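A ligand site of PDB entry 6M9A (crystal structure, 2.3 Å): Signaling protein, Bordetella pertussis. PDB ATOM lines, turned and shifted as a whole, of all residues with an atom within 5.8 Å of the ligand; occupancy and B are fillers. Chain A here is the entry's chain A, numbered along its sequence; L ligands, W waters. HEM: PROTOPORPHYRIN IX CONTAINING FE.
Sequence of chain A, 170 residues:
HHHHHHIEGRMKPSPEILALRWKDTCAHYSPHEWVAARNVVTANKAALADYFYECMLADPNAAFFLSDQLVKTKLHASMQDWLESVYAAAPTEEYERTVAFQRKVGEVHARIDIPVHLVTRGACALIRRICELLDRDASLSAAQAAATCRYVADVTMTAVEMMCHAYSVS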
ATOM      1  N   PHE A  52     -11.985  27.176 -26.511  1.00  0.00           N
ATOM      2  CA  PHE A  52     -10.629  27.299 -25.955  1.00  0.00           C
ATOM      3  C   PHE A  52      -9.871  28.444 -26.623  1.00  0.00           C
ATOM      4  O   PHE A  52      -9.324  29.327 -25.944  1.00  0.00           O
ATOM      5  CB  PHE A  52      -9.875  25.964 -26.072  1.00  0.00           C
ATOM      6  CG  PHE A  52      -8.464  25.976 -25.508  1.00  0.00           C
ATOM      7  CD1 PHE A  52      -8.187  25.379 -24.281  1.00  0.00           C
ATOM      8  CD2 PHE A  52      -7.399  26.551 -26.216  1.00  0.00           C
ATOM      9  CE1 PHE A  52      -6.885  25.395 -23.741  1.00  0.00           C
ATOM     10  CE2 PHE A  52      -6.106  26.557 -25.696  1.00  0.00           C
ATOM     11  CZ  PHE A  52      -5.845  25.984 -24.453  1.00  0.00           C
ATOM     12  N   TYR A  53      -9.849  28.471 -27.960  1.00  0.00           N
ATOM     13  CA  TYR A  53      -9.020  29.448 -28.640  1.00  0.00           C
ATOM     14  C   TYR A  53      -9.643  30.832 -28.712  1.00  0.00           C
ATOM     15  O   TYR A  53      -8.917  31.812 -28.845  1.00  0.00           O
ATOM     16  CB  TYR A  53      -8.628  28.928 -30.045  1.00  0.00           C
ATOM     17  CG  TYR A  53      -7.583  27.858 -29.867  1.00  0.00           C
ATOM     18  CD1 TYR A  53      -6.292  28.200 -29.467  1.00  0.00           C
ATOM     19  CD2 TYR A  53      -7.892  26.516 -30.000  1.00  0.00           C
ATOM     20  CE1 TYR A  53      -5.325  27.226 -29.245  1.00  0.00           C
ATOM     21  CE2 TYR A  53      -6.919  25.523 -29.781  1.00  0.00           C
ATOM     22  CZ  TYR A  53      -5.641  25.898 -29.405  1.00  0.00           C
ATOM     23  OH  TYR A  53      -4.690  24.948 -29.167  1.00  0.00           O
ATOM     24  N   MET A  56      -8.353  32.281 -25.384  1.00  0.00           N
ATOM     25  CA  MET A  56      -6.939  32.616 -25.464  1.00  0.00           C
ATOM     26  C   MET A  56      -6.679  33.810 -26.393  1.00  0.00           C
ATOM     27  O   MET A  56      -5.902  34.702 -26.056  1.00  0.00           O
ATOM     28  CB  MET A  56      -6.147  31.396 -25.939  1.00  0.00           C
ATOM     29  CG  MET A  56      -6.055  30.262 -24.904  1.00  0.00           C
ATOM     30  SD  MET A  56      -5.297  30.826 -23.371  1.00  0.00           S
ATOM     31  CE  MET A  56      -5.665  29.451 -22.314  1.00  0.00           C
ATOM     32  N   ALA A  62      -2.052  36.217 -23.687  1.00  0.00           N
ATOM     33  CA  ALA A  62      -1.993  34.913 -24.342  1.00  0.00           C
ATOM     34  C   ALA A  62      -1.965  35.049 -25.870  1.00  0.00           C
ATOM     35  O   ALA A  62      -1.321  34.233 -26.546  1.00  0.00           O
ATOM     36  CB  ALA A  62      -3.187  34.065 -23.914  1.00  0.00           C
ATOM     37  N   ALA A  63      -2.616  36.072 -26.402  1.00  0.00           N
ATOM     38  CA  ALA A  63      -2.623  36.288 -27.843  1.00  0.00           C
ATOM     39  C   ALA A  63      -1.218  36.604 -28.321  1.00  0.00           C
ATOM     40  O   ALA A  63      -0.972  36.639 -29.519  1.00  0.00           O
ATOM     41  CB  ALA A  63      -3.579  37.407 -28.212  1.00  0.00           C
ATOM     42  N   PHE A  65       1.420  34.757 -27.904  1.00  0.00           N
ATOM     43  CA  PHE A  65       2.004  33.497 -28.371  1.00  0.00           C
ATOM     44  C   PHE A  65       1.237  32.867 -29.534  1.00  0.00           C
ATOM     45  O   PHE A  65       1.664  31.824 -30.052  1.00  0.00           O
ATOM     46  CB  PHE A  65       2.077  32.514 -27.202  1.00  0.00           C
ATOM     47  CG  PHE A  65       2.809  33.064 -26.003  1.00  0.00           C
ATOM     48  CD1 PHE A  65       4.182  32.954 -25.898  1.00  0.00           C
ATOM     49  CD2 PHE A  65       2.126  33.728 -24.994  1.00  0.00           C
ATOM     50  CE1 PHE A  65       4.867  33.479 -24.807  1.00  0.00           C
ATOM     51  CE2 PHE A  65       2.797  34.260 -23.910  1.00  0.00           C
ATOM     52  CZ  PHE A  65       4.162  34.138 -23.815  1.00  0.00           C
ATOM     53  N   LEU A  66       0.114  33.443 -29.967  1.00  0.00           N
ATOM     54  CA  LEU A  66      -0.725  32.830 -30.983  1.00  0.00           C
ATOM     55  C   LEU A  66      -0.891  33.760 -32.185  1.00  0.00           C
ATOM     56  O   LEU A  66      -1.176  34.951 -32.039  1.00  0.00           O
ATOM     57  CB  LEU A  66      -2.096  32.476 -30.413  1.00  0.00           C
ATOM     58  CG  LEU A  66      -2.010  31.533 -29.210  1.00  0.00           C
ATOM     59  CD1 LEU A  66      -3.362  31.437 -28.518  1.00  0.00           C
ATOM     60  CD2 LEU A  66      -1.512  30.175 -29.677  1.00  0.00           C
ATOM     61  N   LEU A  70      -1.863  30.052 -36.985  1.00  0.00           N
ATOM     62  CA  LEU A  70      -1.471  28.856 -36.250  1.00  0.00           C
ATOM     63  C   LEU A  70      -2.691  28.146 -35.688  1.00  0.00           C
ATOM     64  O   LEU A  70      -2.805  26.913 -35.756  1.00  0.00           O
ATOM     65  CB  LEU A  70      -0.491  29.251 -35.141  1.00  0.00           C
ATOM     66  CG  LEU A  70       0.184  28.169 -34.294  1.00  0.00           C
ATOM     67  CD1 LEU A  70       0.991  27.249 -35.193  1.00  0.00           C
ATOM     68  CD2 LEU A  70       1.067  28.828 -33.227  1.00  0.00           C
ATOM     69  N   LYS A  74      -3.468  24.635 -37.462  1.00  0.00           N
ATOM     70  CA  LYS A  74      -2.768  23.616 -36.693  1.00  0.00           C
ATOM     71  C   LYS A  74      -3.418  23.343 -35.339  1.00  0.00           C
ATOM     72  O   LYS A  74      -3.841  22.218 -35.079  1.00  0.00           O
ATOM     73  CB  LYS A  74      -1.305  23.994 -36.520  1.00  0.00           C
ATOM     74  CG  LYS A  74      -0.491  22.970 -35.769  1.00  0.00           C
ATOM     75  CD  LYS A  74       0.964  23.383 -35.753  1.00  0.00           C
ATOM     76  CE  LYS A  74       1.820  22.316 -35.117  1.00  0.00           C
ATOM     77  NZ  LYS A  74       3.241  22.412 -35.575  1.00  0.00           N
ATOM     78  N   LEU A  75      -3.547  24.371 -34.483  1.00  0.00           N
ATOM     79  CA  LEU A  75      -3.892  24.116 -33.094  1.00  0.00           C
ATOM     80  C   LEU A  75      -5.360  23.758 -32.906  1.00  0.00           C
ATOM     81  O   LEU A  75      -5.686  22.980 -31.995  1.00  0.00           O
ATOM     82  CB  LEU A  75      -3.572  25.307 -32.196  1.00  0.00           C
ATOM     83  CG  LEU A  75      -2.128  25.769 -32.234  1.00  0.00           C
ATOM     84  CD1 LEU A  75      -1.956  26.968 -31.322  1.00  0.00           C
ATOM     85  CD2 LEU A  75      -1.237  24.596 -31.841  1.00  0.00           C
ATOM     86  N   SER A  78      -5.185  20.149 -33.395  1.00  0.00           N
ATOM     87  CA  SER A  78      -4.371  19.470 -32.386  1.00  0.00           C
ATOM     88  C   SER A  78      -5.068  19.449 -31.043  1.00  0.00           C
ATOM     89  O   SER A  78      -4.914  18.495 -30.271  1.00  0.00           O
ATOM     90  CB  SER A  78      -3.022  20.169 -32.245  1.00  0.00           C
ATOM     91  OG  SER A  78      -2.529  20.573 -33.517  1.00  0.00           O
ATOM     92  N   MET A  79      -5.825  20.496 -30.728  1.00  0.00           N
ATOM     93  CA  MET A  79      -6.599  20.514 -29.491  1.00  0.00           C
ATOM     94  C   MET A  79      -7.693  19.435 -29.517  1.00  0.00           C
ATOM     95  O   MET A  79      -7.934  18.760 -28.513  1.00  0.00           O
ATOM     96  CB  MET A  79      -7.216  21.891 -29.268  1.00  0.00           C
ATOM     97  CG  MET A  79      -8.203  21.955 -28.104  1.00  0.00           C
ATOM     98  SD  MET A  79      -7.428  21.595 -26.507  1.00  0.00           S
ATOM     99  CE  MET A  79      -6.314  22.989 -26.383  1.00  0.00           C
ATOM    100  N   TRP A  82      -6.041  16.230 -28.861  1.00  0.00           N
ATOM    101  CA  TRP A  82      -5.573  16.168 -27.484  1.00  0.00           C
ATOM    102  C   TRP A  82      -6.710  15.736 -26.563  1.00  0.00           C
ATOM    103  O   TRP A  82      -6.544  14.837 -25.724  1.00  0.00           O
ATOM    104  CB  TRP A  82      -4.990  17.518 -27.067  1.00  0.00           C
ATOM    105  CG  TRP A  82      -4.454  17.554 -25.658  1.00  0.00           C
ATOM    106  CD1 TRP A  82      -3.174  17.314 -25.258  1.00  0.00           C
ATOM    107  CD2 TRP A  82      -5.198  17.832 -24.473  1.00  0.00           C
ATOM    108  NE1 TRP A  82      -3.083  17.442 -23.899  1.00  0.00           N
ATOM    109  CE2 TRP A  82      -4.314  17.740 -23.391  1.00  0.00           C
ATOM    110  CE3 TRP A  82      -6.547  18.140 -24.220  1.00  0.00           C
ATOM    111  CZ2 TRP A  82      -4.709  17.966 -22.064  1.00  0.00           C
ATOM    112  CZ3 TRP A  82      -6.944  18.368 -22.904  1.00  0.00           C
ATOM    113  CH2 TRP A  82      -6.025  18.290 -21.845  1.00  0.00           C
ATOM    114  N   PHE A 101       2.640  11.099 -24.637  1.00  0.00           N
ATOM    115  CA  PHE A 101       2.132  12.201 -25.446  1.00  0.00           C
ATOM    116  C   PHE A 101       1.974  13.487 -24.604  1.00  0.00           C
ATOM    117  O   PHE A 101       2.401  14.569 -25.034  1.00  0.00           O
ATOM    118  CB  PHE A 101       0.818  11.776 -26.078  1.00  0.00           C
ATOM    119  CG  PHE A 101       0.062  12.879 -26.756  1.00  0.00           C
ATOM    120  CD1 PHE A 101       0.512  13.415 -27.953  1.00  0.00           C
ATOM    121  CD2 PHE A 101      -1.109  13.376 -26.201  1.00  0.00           C
ATOM    122  CE1 PHE A 101      -0.187  14.421 -28.581  1.00  0.00           C
ATOM    123  CE2 PHE A 101      -1.809  14.381 -26.829  1.00  0.00           C
ATOM    124  CZ  PHE A 101      -1.344  14.909 -28.019  1.00  0.00           C
ATOM    125  N   VAL A 105       3.870  17.099 -25.280  1.00  0.00           N
ATOM    126  CA  VAL A 105       3.076  18.329 -25.416  1.00  0.00           C
ATOM    127  C   VAL A 105       3.560  19.370 -24.411  1.00  0.00           C
ATOM    128  O   VAL A 105       3.814  20.528 -24.773  1.00  0.00           O
ATOM    129  CB  VAL A 105       1.584  18.009 -25.240  1.00  0.00           C
ATOM    130  CG1 VAL A 105       0.793  19.293 -24.951  1.00  0.00           C
ATOM    131  CG2 VAL A 105       1.074  17.241 -26.462  1.00  0.00           C
ATOM    132  N   VAL A 108       6.643  21.133 -25.542  1.00  0.00           N
ATOM    133  CA  VAL A 108       6.515  22.134 -26.598  1.00  0.00           C
ATOM    134  C   VAL A 108       6.214  23.516 -26.006  1.00  0.00           C
ATOM    135  O   VAL A 108       6.707  24.540 -26.474  1.00  0.00           O
ATOM    136  CB  VAL A 108       5.440  21.707 -27.615  1.00  0.00           C
ATOM    137  CG1 VAL A 108       5.037  22.875 -28.514  1.00  0.00           C
ATOM    138  CG2 VAL A 108       5.950  20.543 -28.456  1.00  0.00           C
ATOM    139  N   HIS A 109       5.426  23.549 -24.938  1.00  0.00           N
ATOM    140  CA  HIS A 109       5.059  24.813 -24.321  1.00  0.00           C
ATOM    141  C   HIS A 109       6.197  25.399 -23.508  1.00  0.00           C
ATOM    142  O   HIS A 109       6.442  26.606 -23.556  1.00  0.00           O
ATOM    143  CB  HIS A 109       3.803  24.602 -23.475  1.00  0.00           C
ATOM    144  CG  HIS A 109       2.596  24.272 -24.295  1.00  0.00           C
ATOM    145  ND1 HIS A 109       2.174  22.987 -24.515  1.00  0.00           N
ATOM    146  CD2 HIS A 109       1.750  25.077 -24.987  1.00  0.00           C
ATOM    147  CE1 HIS A 109       1.110  22.996 -25.294  1.00  0.00           C
ATOM    148  NE2 HIS A 109       0.813  24.259 -25.586  1.00  0.00           N
ATOM    149  N   ILE A 112       8.986  27.103 -25.753  1.00  0.00           N
ATOM    150  CA  ILE A 112       8.702  28.462 -26.219  1.00  0.00           C
ATOM    151  C   ILE A 112       8.223  29.364 -25.089  1.00  0.00           C
ATOM    152  O   ILE A 112       7.834  30.498 -25.342  1.00  0.00           O
ATOM    153  CB  ILE A 112       7.692  28.458 -27.375  1.00  0.00           C
ATOM    154  CG1 ILE A 112       6.438  27.684 -26.990  1.00  0.00           C
ATOM    155  CG2 ILE A 112       8.314  27.862 -28.632  1.00  0.00           C
ATOM    156  CD1 ILE A 112       5.532  27.372 -28.151  1.00  0.00           C
ATOM    157  N   ILE A 114       5.564  29.287 -22.952  1.00  0.00           N
ATOM    158  CA  ILE A 114       4.165  29.573 -22.653  1.00  0.00           C
ATOM    159  C   ILE A 114       4.077  29.663 -21.128  1.00  0.00           C
ATOM    160  O   ILE A 114       4.465  28.705 -20.434  1.00  0.00           O
ATOM    161  CB  ILE A 114       3.219  28.492 -23.213  1.00  0.00           C
ATOM    162  CG1 ILE A 114       3.405  28.323 -24.733  1.00  0.00           C
ATOM    163  CG2 ILE A 114       1.793  28.840 -22.891  1.00  0.00           C
ATOM    164  CD1 ILE A 114       3.289  29.564 -25.516  1.00  0.00           C
ATOM    165  N   PRO A 115       3.614  30.772 -20.566  1.00  0.00           N
ATOM    166  CA  PRO A 115       3.454  30.865 -19.110  1.00  0.00           C
ATOM    167  C   PRO A 115       2.553  29.740 -18.611  1.00  0.00           C
ATOM    168  O   PRO A 115       1.495  29.471 -19.171  1.00  0.00           O
ATOM    169  CB  PRO A 115       2.805  32.236 -18.903  1.00  0.00           C
ATOM    170  CG  PRO A 115       3.148  33.009 -20.125  1.00  0.00           C
ATOM    171  CD  PRO A 115       3.165  32.006 -21.245  1.00  0.00           C
ATOM    172  N   LEU A 118      -1.197  30.248 -17.941  1.00  0.00           N
ATOM    173  CA  LEU A 118      -2.101  30.209 -19.088  1.00  0.00           C
ATOM    174  C   LEU A 118      -2.512  28.778 -19.420  1.00  0.00           C
ATOM    175  O   LEU A 118      -3.676  28.526 -19.768  1.00  0.00           O
ATOM    176  CB  LEU A 118      -1.428  30.874 -20.294  1.00  0.00           C
ATOM    177  CG  LEU A 118      -1.123  32.353 -20.113  1.00  0.00           C
ATOM    178  CD1 LEU A 118      -0.666  32.963 -21.414  1.00  0.00           C
ATOM    179  CD2 LEU A 118      -2.362  33.097 -19.576  1.00  0.00           C
ATOM    180  N   VAL A 119      -1.577  27.827 -19.322  1.00  0.00           N
ATOM    181  CA  VAL A 119      -1.922  26.417 -19.488  1.00  0.00           C
ATOM    182  C   VAL A 119      -2.947  25.976 -18.453  1.00  0.00           C
ATOM    183  O   VAL A 119      -3.933  25.294 -18.762  1.00  0.00           O
ATOM    184  CB  VAL A 119      -0.640  25.560 -19.423  1.00  0.00           C
ATOM    185  CG1 VAL A 119      -0.989  24.100 -19.483  1.00  0.00           C
ATOM    186  CG2 VAL A 119       0.315  25.947 -20.566  1.00  0.00           C
ATOM    187  N   THR A 120      -2.740  26.376 -17.190  1.00  0.00           N
ATOM    188  CA  THR A 120      -3.724  26.113 -16.139  1.00  0.00           C
ATOM    189  C   THR A 120      -5.082  26.693 -16.503  1.00  0.00           C
ATOM    190  O   THR A 120      -6.116  26.013 -16.416  1.00  0.00           O
ATOM    191  CB  THR A 120      -3.237  26.720 -14.822  1.00  0.00           C
ATOM    192  OG1 THR A 120      -2.146  25.933 -14.320  1.00  0.00           O
ATOM    193  CG2 THR A 120      -4.351  26.804 -13.798  1.00  0.00           C
ATOM    194  N   GLY A 122      -6.313  27.460 -19.373  1.00  0.00           N
ATOM    195  CA  GLY A 122      -6.930  26.745 -20.469  1.00  0.00           C
ATOM    196  C   GLY A 122      -7.536  25.422 -20.042  1.00  0.00           C
ATOM    197  O   GLY A 122      -8.644  25.062 -20.463  1.00  0.00           O
ATOM    198  N   ALA A 123      -6.829  24.679 -19.208  1.00  0.00           N
ATOM    199  CA  ALA A 123      -7.410  23.472 -18.617  1.00  0.00           C
ATOM    200  C   ALA A 123      -8.714  23.785 -17.890  1.00  0.00           C
ATOM    201  O   ALA A 123      -9.718  23.083 -18.055  1.00  0.00           O
ATOM    202  CB  ALA A 123      -6.408  22.845 -17.662  1.00  0.00           C
ATOM    203  N   LEU A 126     -11.515  24.232 -20.359  1.00  0.00           N
ATOM    204  CA  LEU A 126     -12.010  22.968 -20.880  1.00  0.00           C
ATOM    205  C   LEU A 126     -12.890  22.253 -19.852  1.00  0.00           C
ATOM    206  O   LEU A 126     -13.928  21.691 -20.209  1.00  0.00           O
ATOM    207  CB  LEU A 126     -10.838  22.062 -21.325  1.00  0.00           C
ATOM    208  CG  LEU A 126     -10.069  22.547 -22.548  1.00  0.00           C
ATOM    209  CD1 LEU A 126      -8.824  21.708 -22.832  1.00  0.00           C
ATOM    210  CD2 LEU A 126     -10.973  22.583 -23.768  1.00  0.00           C
ATOM    211  N   VAL A 160      -2.881  17.767 -17.399  1.00  0.00           N
ATOM    212  CA  VAL A 160      -2.145  19.021 -17.274  1.00  0.00           C
ATOM    213  C   VAL A 160      -0.943  18.858 -16.353  1.00  0.00           C
ATOM    214  O   VAL A 160       0.121  19.455 -16.578  1.00  0.00           O
ATOM    215  CB  VAL A 160      -3.089  20.148 -16.817  1.00  0.00           C
ATOM    216  CG1 VAL A 160      -2.344  21.441 -16.597  1.00  0.00           C
ATOM    217  CG2 VAL A 160      -4.137  20.336 -17.872  1.00  0.00           C
ATOM    218  N   MET A 163       1.670  17.421 -18.533  1.00  0.00           N
ATOM    219  CA  MET A 163       2.183  18.535 -19.309  1.00  0.00           C
ATOM    220  C   MET A 163       3.098  19.412 -18.474  1.00  0.00           C
ATOM    221  O   MET A 163       4.100  19.933 -18.975  1.00  0.00           O
ATOM    222  CB  MET A 163       1.040  19.361 -19.879  1.00  0.00           C
ATOM    223  CG  MET A 163       0.453  18.855 -21.157  1.00  0.00           C
ATOM    224  SD  MET A 163      -0.909  19.911 -21.653  1.00  0.00           S
ATOM    225  CE  MET A 163      -2.159  19.238 -20.622  1.00  0.00           C
HETATM  226  CHA HEM L   1       1.141  23.426 -29.306  1.00  0.00           C
HETATM  227  CHB HEM L   1      -2.504  21.679 -26.583  1.00  0.00           C
HETATM  228  CHC HEM L   1      -2.142  25.619 -23.831  1.00  0.00           C
HETATM  229  CHD HEM L   1       0.079  27.807 -27.558  1.00  0.00           C
HETATM  230  C1A HEM L   1       0.211  22.550 -28.770  1.00  0.00           C
HETATM  231  C2A HEM L   1       0.025  21.148 -29.083  1.00  0.00           C
HETATM  232  C3A HEM L   1      -0.972  20.678 -28.321  1.00  0.00           C
HETATM  233  C4A HEM L   1      -1.478  21.752 -27.502  1.00  0.00           C
HETATM  234  CMA HEM L   1      -1.510  19.239 -28.328  1.00  0.00           C
HETATM  235  CAA HEM L   1       0.841  20.299 -30.076  1.00  0.00           C
HETATM  236  CBA HEM L   1       0.866  20.827 -31.502  1.00  0.00           C
HETATM  237  CGA HEM L   1       1.755  19.864 -32.266  1.00  0.00           C
HETATM  238  O1A HEM L   1       1.487  19.616 -33.470  1.00  0.00           O
HETATM  239  O2A HEM L   1       2.730  19.322 -31.663  1.00  0.00           O
HETATM  240  C1B HEM L   1      -2.646  22.527 -25.503  1.00  0.00           C
HETATM  241  C2B HEM L   1      -3.357  22.276 -24.259  1.00  0.00           C
HETATM  242  C3B HEM L   1      -3.239  23.358 -23.487  1.00  0.00           C
HETATM  243  C4B HEM L   1      -2.475  24.349 -24.237  1.00  0.00           C
HETATM  244  CMB HEM L   1      -4.077  20.946 -23.917  1.00  0.00           C
HETATM  245  CAB HEM L   1      -3.814  23.622 -22.066  1.00  0.00           C
HETATM  246  CBB HEM L   1      -4.887  23.034 -21.542  1.00  0.00           C
HETATM  247  C1C HEM L   1      -1.592  26.600 -24.630  1.00  0.00           C
HETATM  248  C2C HEM L   1      -1.561  28.016 -24.352  1.00  0.00           C
HETATM  249  C3C HEM L   1      -0.926  28.630 -25.385  1.00  0.00           C
HETATM  250  C4C HEM L   1      -0.560  27.615 -26.348  1.00  0.00           C
HETATM  251  CMC HEM L   1      -2.160  28.614 -23.069  1.00  0.00           C
HETATM  252  CAC HEM L   1      -0.648  30.141 -25.614  1.00  0.00           C
HETATM  253  CBC HEM L   1      -1.339  31.141 -25.040  1.00  0.00           C
HETATM  254  C1D HEM L   1       0.682  26.821 -28.300  1.00  0.00           C
HETATM  255  C2D HEM L   1       1.778  26.962 -29.251  1.00  0.00           C
HETATM  256  C3D HEM L   1       2.069  25.759 -29.737  1.00  0.00           C
HETATM  257  C4D HEM L   1       1.186  24.796 -29.107  1.00  0.00           C
HETATM  258  CMD HEM L   1       2.472  28.285 -29.652  1.00  0.00           C
HETATM  259  CAD HEM L   1       3.193  25.468 -30.769  1.00  0.00           C
HETATM  260  CBD HEM L   1       2.634  25.202 -32.163  1.00  0.00           C
HETATM  261  CGD HEM L   1       3.773  25.055 -33.148  1.00  0.00           C
HETATM  262  O1D HEM L   1       4.526  26.033 -33.408  1.00  0.00           O
HETATM  263  O2D HEM L   1       3.941  23.953 -33.693  1.00  0.00           O
HETATM  264  NA  HEM L   1      -0.731  22.872 -27.804  1.00  0.00           N
HETATM  265  NB  HEM L   1      -2.135  23.801 -25.442  1.00  0.00           N
HETATM  266  NC  HEM L   1      -0.969  26.398 -25.847  1.00  0.00           N
HETATM  267  ND  HEM L   1       0.357  25.497 -28.254  1.00  0.00           N
HETATM  268 FE   HEM L   1      -0.834  24.621 -26.809  1.00  0.00          FE
HETATM  269  O   HOH W   1      -3.648  22.264 -29.725  1.00  0.00           O
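NE2 of His 109 binds FE of the ligand, at 2.1 Å. The side-chain amino group of Lys 74 lies within salt-bridge range of an oxygen (O2D) of the ligand (2.5 Å).
O of His 109 lies within hydrogen-bond range of N of Ile 114. A ring nitrogen (ND1) of His 109 sits at hydrogen-bond distance from the backbone carbonyl oxygen (O) of Val 105 (3.0 Å). The side-chain hydroxyl (OG) of Ser 78 lies within hydrogen-bond range of the backbone carbonyl oxygen (O) of Lys 74 (2.6 Å). The backbone carbonyl oxygen (O) of Leu 70 is in hydrogen-bond range of the backbone NH (N) of Leu 75, 2.9 Å away.
Phe 52 touches the ligand. Met 56 touches the ligand. Ala 62 touches the ligand (O to CBC, 3.4 Å). O of Phe 65 touches CMD of the ligand (3.7 Å). Leu 66 touches the ligand (CD2 to CHD, 3.6 Å). CD2 of Leu 70 touches CMD of the ligand (3.9 Å). Leu 75 touches the ligand (CD2 to C4D, 3.7 Å). Ser 78 touches the ligand (OG to CBA, 3.96 Å). Met 79 touches the ligand. Trp 82 touches the ligand (CE2 to CMB, 3.3 Å). Val 105 touches the ligand. CG1 of Val 108 touches CAD of the ligand, 3.9 Å away. Ile 112 touches the ligand (CD1 to CMD, 3.5 Å). Ile 114 touches the ligand. O of Leu 118 touches CMC of the ligand (3.6 Å). Val 119 touches the ligand (O to CAB, 3.7 Å). Gly 122 touches the ligand (C to CBB, 3.9 Å). N of Ala 123 touches CBB of the ligand, at 3.5 Å. Hydrophobic or aromatic side chains within 4 Å of the ligand: Phe 52, Met 56, Ala 62, Phe 65, Leu 66, Leu 70, Leu 75, Met 79, Trp 82, Val 105, Val 108, His 109, Ile 112, Ile 114, Leu 118 and Val 119. Within 4 Å of the ligand: Phe 52, Met 56, Ala 62, Phe 65, Leu 66, Leu 70, Lys 74, Leu 75, Ser 78, Met 79, Trp 82, Val 105, Val 108, His 109, Ile 112, Ile 114, Leu 118, Val 119, Gly 122 and Ala 123.
Water W1 lies within hydrogen-bond range of OH of Tyr 53 (2.9 Å), N of Met 79 (3.0 Å) and O of Leu 75 (3.1 Å).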
